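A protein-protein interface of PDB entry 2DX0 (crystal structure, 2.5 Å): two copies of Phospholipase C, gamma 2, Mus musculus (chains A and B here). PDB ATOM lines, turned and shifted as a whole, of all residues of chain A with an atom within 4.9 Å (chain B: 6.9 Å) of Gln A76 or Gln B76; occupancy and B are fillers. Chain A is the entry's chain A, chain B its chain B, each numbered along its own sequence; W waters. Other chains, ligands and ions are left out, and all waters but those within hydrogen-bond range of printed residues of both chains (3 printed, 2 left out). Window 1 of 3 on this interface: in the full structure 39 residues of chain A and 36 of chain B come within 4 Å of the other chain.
NE2 of Gln A76 sits close to NE2 of Gln B76, 3.3 Å away.
Of the 19 printed residues of chain B, 7 touch a printed residue of chain A.
Printed residues of chain B that touch a printed residue of chain A: Phe B69, Arg B71, Gln B76, His B77, Cys B116, Phe B119 and Leu B121.
Hydrophobic or aromatic side chains of chain B within 4 Å of the printed part of chain A: Phe B69, His B77, Phe B119 and Leu B121.
Printed residues of chain A that touch a printed residue of chain B: Phe A69, Gln A76, Glu A118 and Phe A119.
Along chain A the printed residues that touch a printed residue of chain B span positions 69 to 119.
Water W3 lies within hydrogen-bond range of the side-chain amide oxygen (OE1) of Gln A76, the side-chain amide nitrogen (NE2) of Gln B76 and the backbone NH (N) of His B77.
Water W2 lies within hydrogen-bond range of a ring nitrogen (NE2) of His B77 (2.6 Å), the side-chain amide oxygen (OE1) of Gln A76 (3.0 Å) and the backbone carbonyl oxygen (O) of Val A75 (3.1 Å).
Water W1 bridges O of His A77 and OE1 of Gln B76.
ND1 of His B77 is in hydrogen-bond range of OE1 of Glu B36, at 2.8 Å.
The side-chain sulfur of Cys B116 lies close to the backbone NH of Glu B118, at 3.7 Å.
The backbone NH (N) of Gln B76 sits at hydrogen-bond distance from the backbone carbonyl oxygen (O) of Phe B69 (2.9 Å).
SG of Cys B116 lies close to N of Phe B119 (3.7 Å).
SG of Cys B78 forms a disulfide with SG of Cys B116.
The backbone carbonyl oxygen (O) of Gln A76 lies within hydrogen-bond range of the backbone NH (N) of Phe A69 (3.1 Å).
Leu B121 touches Phe A69 (CD2 to CE1, 3.4 Å).
NE2 of His B77 touches OE1 of Gln A76, 3.9 Å away.
Gln A76 touches Phe B119 (CG to CD2, 3.2 Å).
Phe B69 touches Glu A118.
CG of Arg B71 touches O of Glu A118, 3.5 Å away.
Glu A118 touches Gln B76 (CB to OE1, 3.9 Å).
Phe A119 touches Phe B69.
CZ of Phe A119 touches O of His B77, at 3.9 Å.
CE2 of Phe A119 touches CB of Cys B116 (3.4 Å).
Of chain B, only Gln B76, His B77 and Phe B119 come within 4 Å of Gln A76.
Of chain A, only Gln A76 and Glu A118 come within 4 Å of Gln B76.
Printed residues of chain A within 4 Å of His B77: Gln A76 (3.9 Å) and Phe A119 (3.9 Å).
Printed residues of chain A within 4 Å of Phe B119: Gln A76.
Of the printed residues of chain A, Leu B121 touches Phe A69.
The nearest residue of chain B that does not touch Gln A76 is Glu B118 (6.5 Å).
The nearest residue of chain A that does not touch Gln B76 is Phe A119 (4.1 Å).
The nearest printed residue of chain A that does not touch His B77 is Arg A74 (4.9 Å).
Gln B76 touches its own counterpart, Gln A76.
Glu A118 touches Phe B69, but with the chains exchanged Phe A69 does not touch Glu B118 (6.0 Å).
Glu A118 touches Gln B76, but with the chains exchanged Gln A76 does not touch Glu B118 (6.5 Å).
Phe A119 touches Phe B69, but with the chains exchanged Phe A69 does not touch Phe B119 (4.1 Å).
Of the 10 pairs that touch across the chains among the printed residues, 1 has its exchanged pair printed and touching as well.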
ATOM      1  N   LEU A  67     -20.697  12.670   2.182  1.00  0.00           N
ATOM      2  CA  LEU A  67     -19.660  13.419   1.492  1.00  0.00           C
ATOM      3  C   LEU A  67     -20.390  14.349   0.520  1.00  0.00           C
ATOM      4  O   LEU A  67     -21.169  13.895  -0.316  1.00  0.00           O
ATOM      5  CB  LEU A  67     -18.727  12.448   0.755  1.00  0.00           C
ATOM      6  CG  LEU A  67     -17.514  12.930  -0.052  1.00  0.00           C
ATOM      7  CD1 LEU A  67     -17.968  13.333  -1.417  1.00  0.00           C
ATOM      8  CD2 LEU A  67     -16.795  14.080   0.637  1.00  0.00           C
ATOM      9  N   SER A  68     -20.162  15.650   0.662  1.00  0.00           N
ATOM     10  CA  SER A  68     -20.798  16.646  -0.198  1.00  0.00           C
ATOM     11  C   SER A  68     -19.719  17.432  -0.925  1.00  0.00           C
ATOM     12  O   SER A  68     -18.911  18.108  -0.295  1.00  0.00           O
ATOM     13  CB  SER A  68     -21.638  17.612   0.636  1.00  0.00           C
ATOM     14  OG  SER A  68     -22.600  16.916   1.393  1.00  0.00           O
ATOM     15  N   PHE A  69     -19.709  17.350  -2.249  1.00  0.00           N
ATOM     16  CA  PHE A  69     -18.704  18.056  -3.024  1.00  0.00           C
ATOM     17  C   PHE A  69     -19.299  18.879  -4.154  1.00  0.00           C
ATOM     18  O   PHE A  69     -20.448  18.686  -4.560  1.00  0.00           O
ATOM     19  CB  PHE A  69     -17.679  17.071  -3.583  1.00  0.00           C
ATOM     20  CG  PHE A  69     -18.272  16.035  -4.480  1.00  0.00           C
ATOM     21  CD1 PHE A  69     -18.269  16.205  -5.859  1.00  0.00           C
ATOM     22  CD2 PHE A  69     -18.835  14.884  -3.948  1.00  0.00           C
ATOM     23  CE1 PHE A  69     -18.814  15.239  -6.691  1.00  0.00           C
ATOM     24  CE2 PHE A  69     -19.383  13.915  -4.768  1.00  0.00           C
ATOM     25  CZ  PHE A  69     -19.371  14.092  -6.143  1.00  0.00           C
ATOM     26  N   ARG A  74     -23.026  22.405  -9.308  1.00  0.00           N
ATOM     27  CA  ARG A  74     -23.724  21.231  -8.800  1.00  0.00           C
ATOM     28  C   ARG A  74     -23.108  20.768  -7.483  1.00  0.00           C
ATOM     29  O   ARG A  74     -21.926  20.987  -7.218  1.00  0.00           O
ATOM     30  CB  ARG A  74     -23.646  20.065  -9.797  1.00  0.00           C
ATOM     31  CG  ARG A  74     -24.785  19.965 -10.795  1.00  0.00           C
ATOM     32  CD  ARG A  74     -24.666  20.996 -11.892  1.00  0.00           C
ATOM     33  NE  ARG A  74     -25.782  20.921 -12.830  1.00  0.00           N
ATOM     34  CZ  ARG A  74     -26.056  21.854 -13.736  1.00  0.00           C
ATOM     35  NH1 ARG A  74     -25.293  22.933 -13.820  1.00  0.00           N
ATOM     36  NH2 ARG A  74     -27.094  21.709 -14.552  1.00  0.00           N
ATOM     37  N   VAL A  75     -23.919  20.138  -6.653  1.00  0.00           N
ATOM     38  CA  VAL A  75     -23.442  19.595  -5.398  1.00  0.00           C
ATOM     39  C   VAL A  75     -23.978  18.180  -5.299  1.00  0.00           C
ATOM     40  O   VAL A  75     -25.183  17.963  -5.381  1.00  0.00           O
ATOM     41  CB  VAL A  75     -23.936  20.399  -4.174  1.00  0.00           C
ATOM     42  CG1 VAL A  75     -23.667  19.606  -2.898  1.00  0.00           C
ATOM     43  CG2 VAL A  75     -23.218  21.745  -4.100  1.00  0.00           C
ATOM     44  N   GLN A  76     -23.069  17.218  -5.165  1.00  0.00           N
ATOM     45  CA  GLN A  76     -23.431  15.813  -5.018  1.00  0.00           C
ATOM     46  C   GLN A  76     -23.218  15.402  -3.581  1.00  0.00           C
ATOM     47  O   GLN A  76     -22.328  15.925  -2.905  1.00  0.00           O
ATOM     48  CB  GLN A  76     -22.570  14.928  -5.909  1.00  0.00           C
ATOM     49  CG  GLN A  76     -23.043  14.889  -7.326  1.00  0.00           C
ATOM     50  CD  GLN A  76     -24.405  14.233  -7.456  1.00  0.00           C
ATOM     51  OE1 GLN A  76     -25.308  14.779  -8.097  1.00  0.00           O
ATOM     52  NE2 GLN A  76     -24.560  13.053  -6.850  1.00  0.00           N
ATOM     53  N   HIS A  77     -24.035  14.459  -3.129  1.00  0.00           N
ATOM     54  CA  HIS A  77     -23.960  13.940  -1.773  1.00  0.00           C
ATOM     55  C   HIS A  77     -23.809  12.418  -1.850  1.00  0.00           C
ATOM     56  O   HIS A  77     -24.630  11.722  -2.452  1.00  0.00           O
ATOM     57  CB  HIS A  77     -25.234  14.292  -1.000  1.00  0.00           C
ATOM     58  CG  HIS A  77     -25.551  15.756  -0.979  1.00  0.00           C
ATOM     59  ND1 HIS A  77     -24.817  16.669  -0.255  1.00  0.00           N
ATOM     60  CD2 HIS A  77     -26.523  16.463  -1.600  1.00  0.00           C
ATOM     61  CE1 HIS A  77     -25.324  17.876  -0.430  1.00  0.00           C
ATOM     62  NE2 HIS A  77     -26.359  17.778  -1.243  1.00  0.00           N
ATOM     63  N   CYS A  78     -22.750  11.905  -1.243  1.00  0.00           N
ATOM     64  CA  CYS A  78     -22.492  10.473  -1.239  1.00  0.00           C
ATOM     65  C   CYS A  78     -22.474   9.965   0.192  1.00  0.00           C
ATOM     66  O   CYS A  78     -21.728  10.478   1.026  1.00  0.00           O
ATOM     67  CB  CYS A  78     -21.148  10.189  -1.910  1.00  0.00           C
ATOM     68  SG  CYS A  78     -21.142  10.662  -3.667  1.00  0.00           S
ATOM     69  N   GLU A 118     -24.792   5.756  -4.546  1.00  0.00           N
ATOM     70  CA  GLU A 118     -26.048   6.235  -5.111  1.00  0.00           C
ATOM     71  C   GLU A 118     -26.143   5.942  -6.600  1.00  0.00           C
ATOM     72  O   GLU A 118     -27.195   6.133  -7.207  1.00  0.00           O
ATOM     73  CB  GLU A 118     -26.282   7.745  -4.868  1.00  0.00           C
ATOM     74  CG  GLU A 118     -25.206   8.533  -4.120  1.00  0.00           C
ATOM     75  CD  GLU A 118     -24.937   8.040  -2.707  1.00  0.00           C
ATOM     76  OE1 GLU A 118     -23.967   7.286  -2.528  1.00  0.00           O
ATOM     77  OE2 GLU A 118     -25.689   8.403  -1.778  1.00  0.00           O
ATOM     78  N   PHE A 119     -25.048   5.472  -7.190  1.00  0.00           N
ATOM     79  CA  PHE A 119     -25.047   5.141  -8.611  1.00  0.00           C
ATOM     80  C   PHE A 119     -24.825   3.648  -8.833  1.00  0.00           C
ATOM     81  O   PHE A 119     -24.839   3.175  -9.969  1.00  0.00           O
ATOM     82  CB  PHE A 119     -23.977   5.947  -9.360  1.00  0.00           C
ATOM     83  CG  PHE A 119     -24.321   7.396  -9.528  1.00  0.00           C
ATOM     84  CD1 PHE A 119     -24.177   8.291  -8.474  1.00  0.00           C
ATOM     85  CD2 PHE A 119     -24.824   7.869 -10.740  1.00  0.00           C
ATOM     86  CE1 PHE A 119     -24.530   9.636  -8.621  1.00  0.00           C
ATOM     87  CE2 PHE A 119     -25.182   9.216 -10.896  1.00  0.00           C
ATOM     88  CZ  PHE A 119     -25.034  10.097  -9.836  1.00  0.00           C
ATOM     89  N   GLU B  36     -37.897  16.993 -11.566  1.00  0.00           N
ATOM     90  CA  GLU B  36     -37.305  16.542 -10.312  1.00  0.00           C
ATOM     91  C   GLU B  36     -38.439  16.308  -9.315  1.00  0.00           C
ATOM     92  O   GLU B  36     -38.377  15.406  -8.478  1.00  0.00           O
ATOM     93  CB  GLU B  36     -36.350  17.614  -9.773  1.00  0.00           C
ATOM     94  CG  GLU B  36     -35.084  17.085  -9.100  1.00  0.00           C
ATOM     95  CD  GLU B  36     -34.051  16.558 -10.092  1.00  0.00           C
ATOM     96  OE1 GLU B  36     -32.918  16.242  -9.671  1.00  0.00           O
ATOM     97  OE2 GLU B  36     -34.369  16.457 -11.295  1.00  0.00           O
ATOM     98  N   LEU B  39     -40.872  13.127 -10.341  1.00  0.00           N
ATOM     99  CA  LEU B  39     -40.316  11.878  -9.828  1.00  0.00           C
ATOM    100  C   LEU B  39     -40.595  11.770  -8.339  1.00  0.00           C
ATOM    101  O   LEU B  39     -40.983  10.714  -7.840  1.00  0.00           O
ATOM    102  CB  LEU B  39     -38.804  11.822 -10.059  1.00  0.00           C
ATOM    103  CG  LEU B  39     -38.288  11.138 -11.325  1.00  0.00           C
ATOM    104  CD1 LEU B  39     -36.774  11.217 -11.364  1.00  0.00           C
ATOM    105  CD2 LEU B  39     -38.734   9.691 -11.337  1.00  0.00           C
ATOM    106  N   LEU B  54     -36.498   8.989 -15.740  1.00  0.00           N
ATOM    107  CA  LEU B  54     -37.097   9.720 -16.840  1.00  0.00           C
ATOM    108  C   LEU B  54     -35.951  10.523 -17.443  1.00  0.00           C
ATOM    109  O   LEU B  54     -35.036  10.944 -16.736  1.00  0.00           O
ATOM    110  CB  LEU B  54     -38.211  10.656 -16.367  1.00  0.00           C
ATOM    111  CG  LEU B  54     -37.801  12.036 -15.863  1.00  0.00           C
ATOM    112  CD1 LEU B  54     -39.043  12.862 -15.591  1.00  0.00           C
ATOM    113  CD2 LEU B  54     -36.962  11.891 -14.613  1.00  0.00           C
ATOM    114  N   THR B  66     -30.804  15.028 -19.827  1.00  0.00           N
ATOM    115  CA  THR B  66     -30.461  14.810 -18.433  1.00  0.00           C
ATOM    116  C   THR B  66     -31.215  13.587 -17.959  1.00  0.00           C
ATOM    117  O   THR B  66     -32.402  13.440 -18.230  1.00  0.00           O
ATOM    118  CB  THR B  66     -30.847  16.009 -17.548  1.00  0.00           C
ATOM    119  OG1 THR B  66     -29.992  17.120 -17.855  1.00  0.00           O
ATOM    120  CG2 THR B  66     -30.698  15.651 -16.076  1.00  0.00           C
ATOM    121  N   LEU B  67     -30.520  12.704 -17.258  1.00  0.00           N
ATOM    122  CA  LEU B  67     -31.136  11.498 -16.739  1.00  0.00           C
ATOM    123  C   LEU B  67     -31.412  11.705 -15.256  1.00  0.00           C
ATOM    124  O   LEU B  67     -30.544  12.158 -14.520  1.00  0.00           O
ATOM    125  CB  LEU B  67     -30.197  10.310 -16.982  1.00  0.00           C
ATOM    126  CG  LEU B  67     -30.568   8.877 -16.579  1.00  0.00           C
ATOM    127  CD1 LEU B  67     -30.119   8.646 -15.168  1.00  0.00           C
ATOM    128  CD2 LEU B  67     -32.064   8.615 -16.746  1.00  0.00           C
ATOM    129  N   SER B  68     -32.634  11.405 -14.830  1.00  0.00           N
ATOM    130  CA  SER B  68     -33.017  11.550 -13.424  1.00  0.00           C
ATOM    131  C   SER B  68     -33.622  10.246 -12.926  1.00  0.00           C
ATOM    132  O   SER B  68     -34.480   9.660 -13.590  1.00  0.00           O
ATOM    133  CB  SER B  68     -34.041  12.681 -13.238  1.00  0.00           C
ATOM    134  OG  SER B  68     -33.478  13.961 -13.469  1.00  0.00           O
ATOM    135  N   PHE B  69     -33.180   9.792 -11.759  1.00  0.00           N
ATOM    136  CA  PHE B  69     -33.704   8.555 -11.210  1.00  0.00           C
ATOM    137  C   PHE B  69     -33.890   8.575  -9.702  1.00  0.00           C
ATOM    138  O   PHE B  69     -33.248   9.345  -8.987  1.00  0.00           O
ATOM    139  CB  PHE B  69     -32.819   7.372 -11.624  1.00  0.00           C
ATOM    140  CG  PHE B  69     -31.392   7.493 -11.182  1.00  0.00           C
ATOM    141  CD1 PHE B  69     -30.969   6.922  -9.987  1.00  0.00           C
ATOM    142  CD2 PHE B  69     -30.464   8.157 -11.972  1.00  0.00           C
ATOM    143  CE1 PHE B  69     -29.635   7.007  -9.587  1.00  0.00           C
ATOM    144  CE2 PHE B  69     -29.131   8.250 -11.584  1.00  0.00           C
ATOM    145  CZ  PHE B  69     -28.714   7.672 -10.389  1.00  0.00           C
ATOM    146  N   TRP B  70     -34.793   7.717  -9.241  1.00  0.00           N
ATOM    147  CA  TRP B  70     -35.124   7.585  -7.833  1.00  0.00           C
ATOM    148  C   TRP B  70     -34.096   6.715  -7.126  1.00  0.00           C
ATOM    149  O   TRP B  70     -33.785   5.612  -7.580  1.00  0.00           O
ATOM    150  CB  TRP B  70     -36.509   6.964  -7.688  1.00  0.00           C
ATOM    151  CG  TRP B  70     -36.988   6.964  -6.284  1.00  0.00           C
ATOM    152  CD1 TRP B  70     -37.181   5.879  -5.478  1.00  0.00           C
ATOM    153  CD2 TRP B  70     -37.306   8.114  -5.498  1.00  0.00           C
ATOM    154  NE1 TRP B  70     -37.601   6.285  -4.234  1.00  0.00           N
ATOM    155  CE2 TRP B  70     -37.687   7.653  -4.218  1.00  0.00           C
ATOM    156  CE3 TRP B  70     -37.306   9.494  -5.749  1.00  0.00           C
ATOM    157  CZ2 TRP B  70     -38.062   8.522  -3.190  1.00  0.00           C
ATOM    158  CZ3 TRP B  70     -37.678  10.359  -4.725  1.00  0.00           C
ATOM    159  CH2 TRP B  70     -38.052   9.869  -3.461  1.00  0.00           C
ATOM    160  N   ARG B  71     -33.585   7.203  -6.000  1.00  0.00           N
ATOM    161  CA  ARG B  71     -32.568   6.468  -5.258  1.00  0.00           C
ATOM    162  C   ARG B  71     -32.566   6.821  -3.773  1.00  0.00           C
ATOM    163  O   ARG B  71     -32.145   7.914  -3.380  1.00  0.00           O
ATOM    164  CB  ARG B  71     -31.191   6.760  -5.869  1.00  0.00           C
ATOM    165  CG  ARG B  71     -30.016   6.069  -5.208  1.00  0.00           C
ATOM    166  CD  ARG B  71     -30.160   4.561  -5.223  1.00  0.00           C
ATOM    167  NE  ARG B  71     -28.879   3.912  -4.968  1.00  0.00           N
ATOM    168  CZ  ARG B  71     -28.736   2.624  -4.672  1.00  0.00           C
ATOM    169  NH1 ARG B  71     -29.801   1.836  -4.588  1.00  0.00           N
ATOM    170  NH2 ARG B  71     -27.523   2.123  -4.472  1.00  0.00           N
ATOM    171  N   SER B  72     -33.049   5.889  -2.957  1.00  0.00           N
ATOM    172  CA  SER B  72     -33.097   6.069  -1.511  1.00  0.00           C
ATOM    173  C   SER B  72     -33.694   7.406  -1.066  1.00  0.00           C
ATOM    174  O   SER B  72     -33.039   8.193  -0.379  1.00  0.00           O
ATOM    175  CB  SER B  72     -31.690   5.916  -0.926  1.00  0.00           C
ATOM    176  OG  SER B  72     -31.131   4.662  -1.282  1.00  0.00           O
ATOM    177  N   ARG B  74     -34.051  10.097  -2.521  1.00  0.00           N
ATOM    178  CA  ARG B  74     -33.575  11.263  -3.264  1.00  0.00           C
ATOM    179  C   ARG B  74     -33.651  11.054  -4.775  1.00  0.00           C
ATOM    180  O   ARG B  74     -33.653   9.924  -5.264  1.00  0.00           O
ATOM    181  CB  ARG B  74     -32.118  11.592  -2.891  1.00  0.00           C
ATOM    182  CG  ARG B  74     -31.904  12.507  -1.676  1.00  0.00           C
ATOM    183  CD  ARG B  74     -32.298  11.841  -0.371  1.00  0.00           C
ATOM    184  NE  ARG B  74     -31.873  12.593   0.811  1.00  0.00           N
ATOM    185  CZ  ARG B  74     -32.203  13.857   1.073  1.00  0.00           C
ATOM    186  NH1 ARG B  74     -32.968  14.539   0.230  1.00  0.00           N
ATOM    187  NH2 ARG B  74     -31.771  14.437   2.191  1.00  0.00           N
ATOM    188  N   VAL B  75     -33.728  12.160  -5.507  1.00  0.00           N
ATOM    189  CA  VAL B  75     -33.747  12.118  -6.958  1.00  0.00           C
ATOM    190  C   VAL B  75     -32.334  12.479  -7.402  1.00  0.00           C
ATOM    191  O   VAL B  75     -31.853  13.579  -7.130  1.00  0.00           O
ATOM    192  CB  VAL B  75     -34.731  13.148  -7.547  1.00  0.00           C
ATOM    193  CG1 VAL B  75     -34.513  13.281  -9.055  1.00  0.00           C
ATOM    194  CG2 VAL B  75     -36.154  12.722  -7.261  1.00  0.00           C
ATOM    195  N   GLN B  76     -31.661  11.542  -8.060  1.00  0.00           N
ATOM    196  CA  GLN B  76     -30.308  11.782  -8.541  1.00  0.00           C
ATOM    197  C   GLN B  76     -30.383  12.136 -10.016  1.00  0.00           C
ATOM    198  O   GLN B  76     -31.425  12.002 -10.644  1.00  0.00           O
ATOM    199  CB  GLN B  76     -29.439  10.534  -8.362  1.00  0.00           C
ATOM    200  CG  GLN B  76     -29.325  10.059  -6.923  1.00  0.00           C
ATOM    201  CD  GLN B  76     -28.429  10.941  -6.073  1.00  0.00           C
ATOM    202  OE1 GLN B  76     -28.519  10.929  -4.847  1.00  0.00           O
ATOM    203  NE2 GLN B  76     -27.552  11.703  -6.719  1.00  0.00           N
ATOM    204  N   HIS B  77     -29.272  12.594 -10.568  1.00  0.00           N
ATOM    205  CA  HIS B  77     -29.241  12.949 -11.971  1.00  0.00           C
ATOM    206  C   HIS B  77     -27.837  12.882 -12.520  1.00  0.00           C
ATOM    207  O   HIS B  77     -26.857  12.893 -11.774  1.00  0.00           O
ATOM    208  CB  HIS B  77     -29.824  14.352 -12.181  1.00  0.00           C
ATOM    209  CG  HIS B  77     -29.361  15.353 -11.171  1.00  0.00           C
ATOM    210  ND1 HIS B  77     -30.236  16.124 -10.435  1.00  0.00           N
ATOM    211  CD2 HIS B  77     -28.118  15.694 -10.756  1.00  0.00           C
ATOM    212  CE1 HIS B  77     -29.552  16.894  -9.607  1.00  0.00           C
ATOM    213  NE2 HIS B  77     -28.265  16.652  -9.783  1.00  0.00           N
ATOM    214  N   CYS B  78     -27.755  12.787 -13.839  1.00  0.00           N
ATOM    215  CA  CYS B  78     -26.479  12.738 -14.528  1.00  0.00           C
ATOM    216  C   CYS B  78     -26.709  13.212 -15.954  1.00  0.00           C
ATOM    217  O   CYS B  78     -27.714  12.872 -16.583  1.00  0.00           O
ATOM    218  CB  CYS B  78     -25.905  11.317 -14.528  1.00  0.00           C
ATOM    219  SG  CYS B  78     -24.197  11.289 -15.163  1.00  0.00           S
ATOM    220  N   CYS B 116     -21.526   7.503 -14.076  1.00  0.00           N
ATOM    221  CA  CYS B 116     -21.748   8.917 -14.331  1.00  0.00           C
ATOM    222  C   CYS B 116     -20.453   9.715 -14.334  1.00  0.00           C
ATOM    223  O   CYS B 116     -20.008  10.201 -13.291  1.00  0.00           O
ATOM    224  CB  CYS B 116     -22.701   9.484 -13.277  1.00  0.00           C
ATOM    225  SG  CYS B 116     -23.014  11.255 -13.509  1.00  0.00           S
ATOM    226  N   GLU B 118     -19.903  12.571 -15.045  1.00  0.00           N
ATOM    227  CA  GLU B 118     -20.062  13.924 -14.534  1.00  0.00           C
ATOM    228  C   GLU B 118     -19.628  14.003 -13.073  1.00  0.00           C
ATOM    229  O   GLU B 118     -19.046  15.003 -12.635  1.00  0.00           O
ATOM    230  CB  GLU B 118     -21.519  14.379 -14.650  1.00  0.00           C
ATOM    231  CG  GLU B 118     -21.727  15.827 -14.219  1.00  0.00           C
ATOM    232  CD  GLU B 118     -23.174  16.296 -14.319  1.00  0.00           C
ATOM    233  OE1 GLU B 118     -23.399  17.526 -14.244  1.00  0.00           O
ATOM    234  OE2 GLU B 118     -24.083  15.447 -14.465  1.00  0.00           O
ATOM    235  N   PHE B 119     -19.901  12.948 -12.315  1.00  0.00           N
ATOM    236  CA  PHE B 119     -19.549  12.956 -10.908  1.00  0.00           C
ATOM    237  C   PHE B 119     -18.490  11.954 -10.473  1.00  0.00           C
ATOM    238  O   PHE B 119     -18.271  11.760  -9.285  1.00  0.00           O
ATOM    239  CB  PHE B 119     -20.821  12.804 -10.072  1.00  0.00           C
ATOM    240  CG  PHE B 119     -21.825  13.900 -10.314  1.00  0.00           C
ATOM    241  CD1 PHE B 119     -23.082  13.612 -10.842  1.00  0.00           C
ATOM    242  CD2 PHE B 119     -21.495  15.231 -10.048  1.00  0.00           C
ATOM    243  CE1 PHE B 119     -23.998  14.637 -11.107  1.00  0.00           C
ATOM    244  CE2 PHE B 119     -22.401  16.262 -10.308  1.00  0.00           C
ATOM    245  CZ  PHE B 119     -23.654  15.967 -10.838  1.00  0.00           C
ATOM    246  N   LEU B 121     -15.240  12.076 -10.305  1.00  0.00           N
ATOM    247  CA  LEU B 121     -14.054  12.912 -10.320  1.00  0.00           C
ATOM    248  C   LEU B 121     -13.305  12.740  -9.010  1.00  0.00           C
ATOM    249  O   LEU B 121     -13.745  12.015  -8.121  1.00  0.00           O
ATOM    250  CB  LEU B 121     -14.449  14.382 -10.498  1.00  0.00           C
ATOM    251  CG  LEU B 121     -15.188  15.049  -9.331  1.00  0.00           C
ATOM    252  CD1 LEU B 121     -15.504  16.492  -9.678  1.00  0.00           C
ATOM    253  CD2 LEU B 121     -16.468  14.296  -9.034  1.00  0.00           C
HETATM  254  O   HOH W   1     -27.361  11.460  -2.158  1.00  0.00           O
HETATM  255  O   HOH W   2     -26.389  17.580  -8.249  1.00  0.00           O
HETATM  256  O   HOH W   3     -27.400  13.471  -8.601  1.00  0.00           O
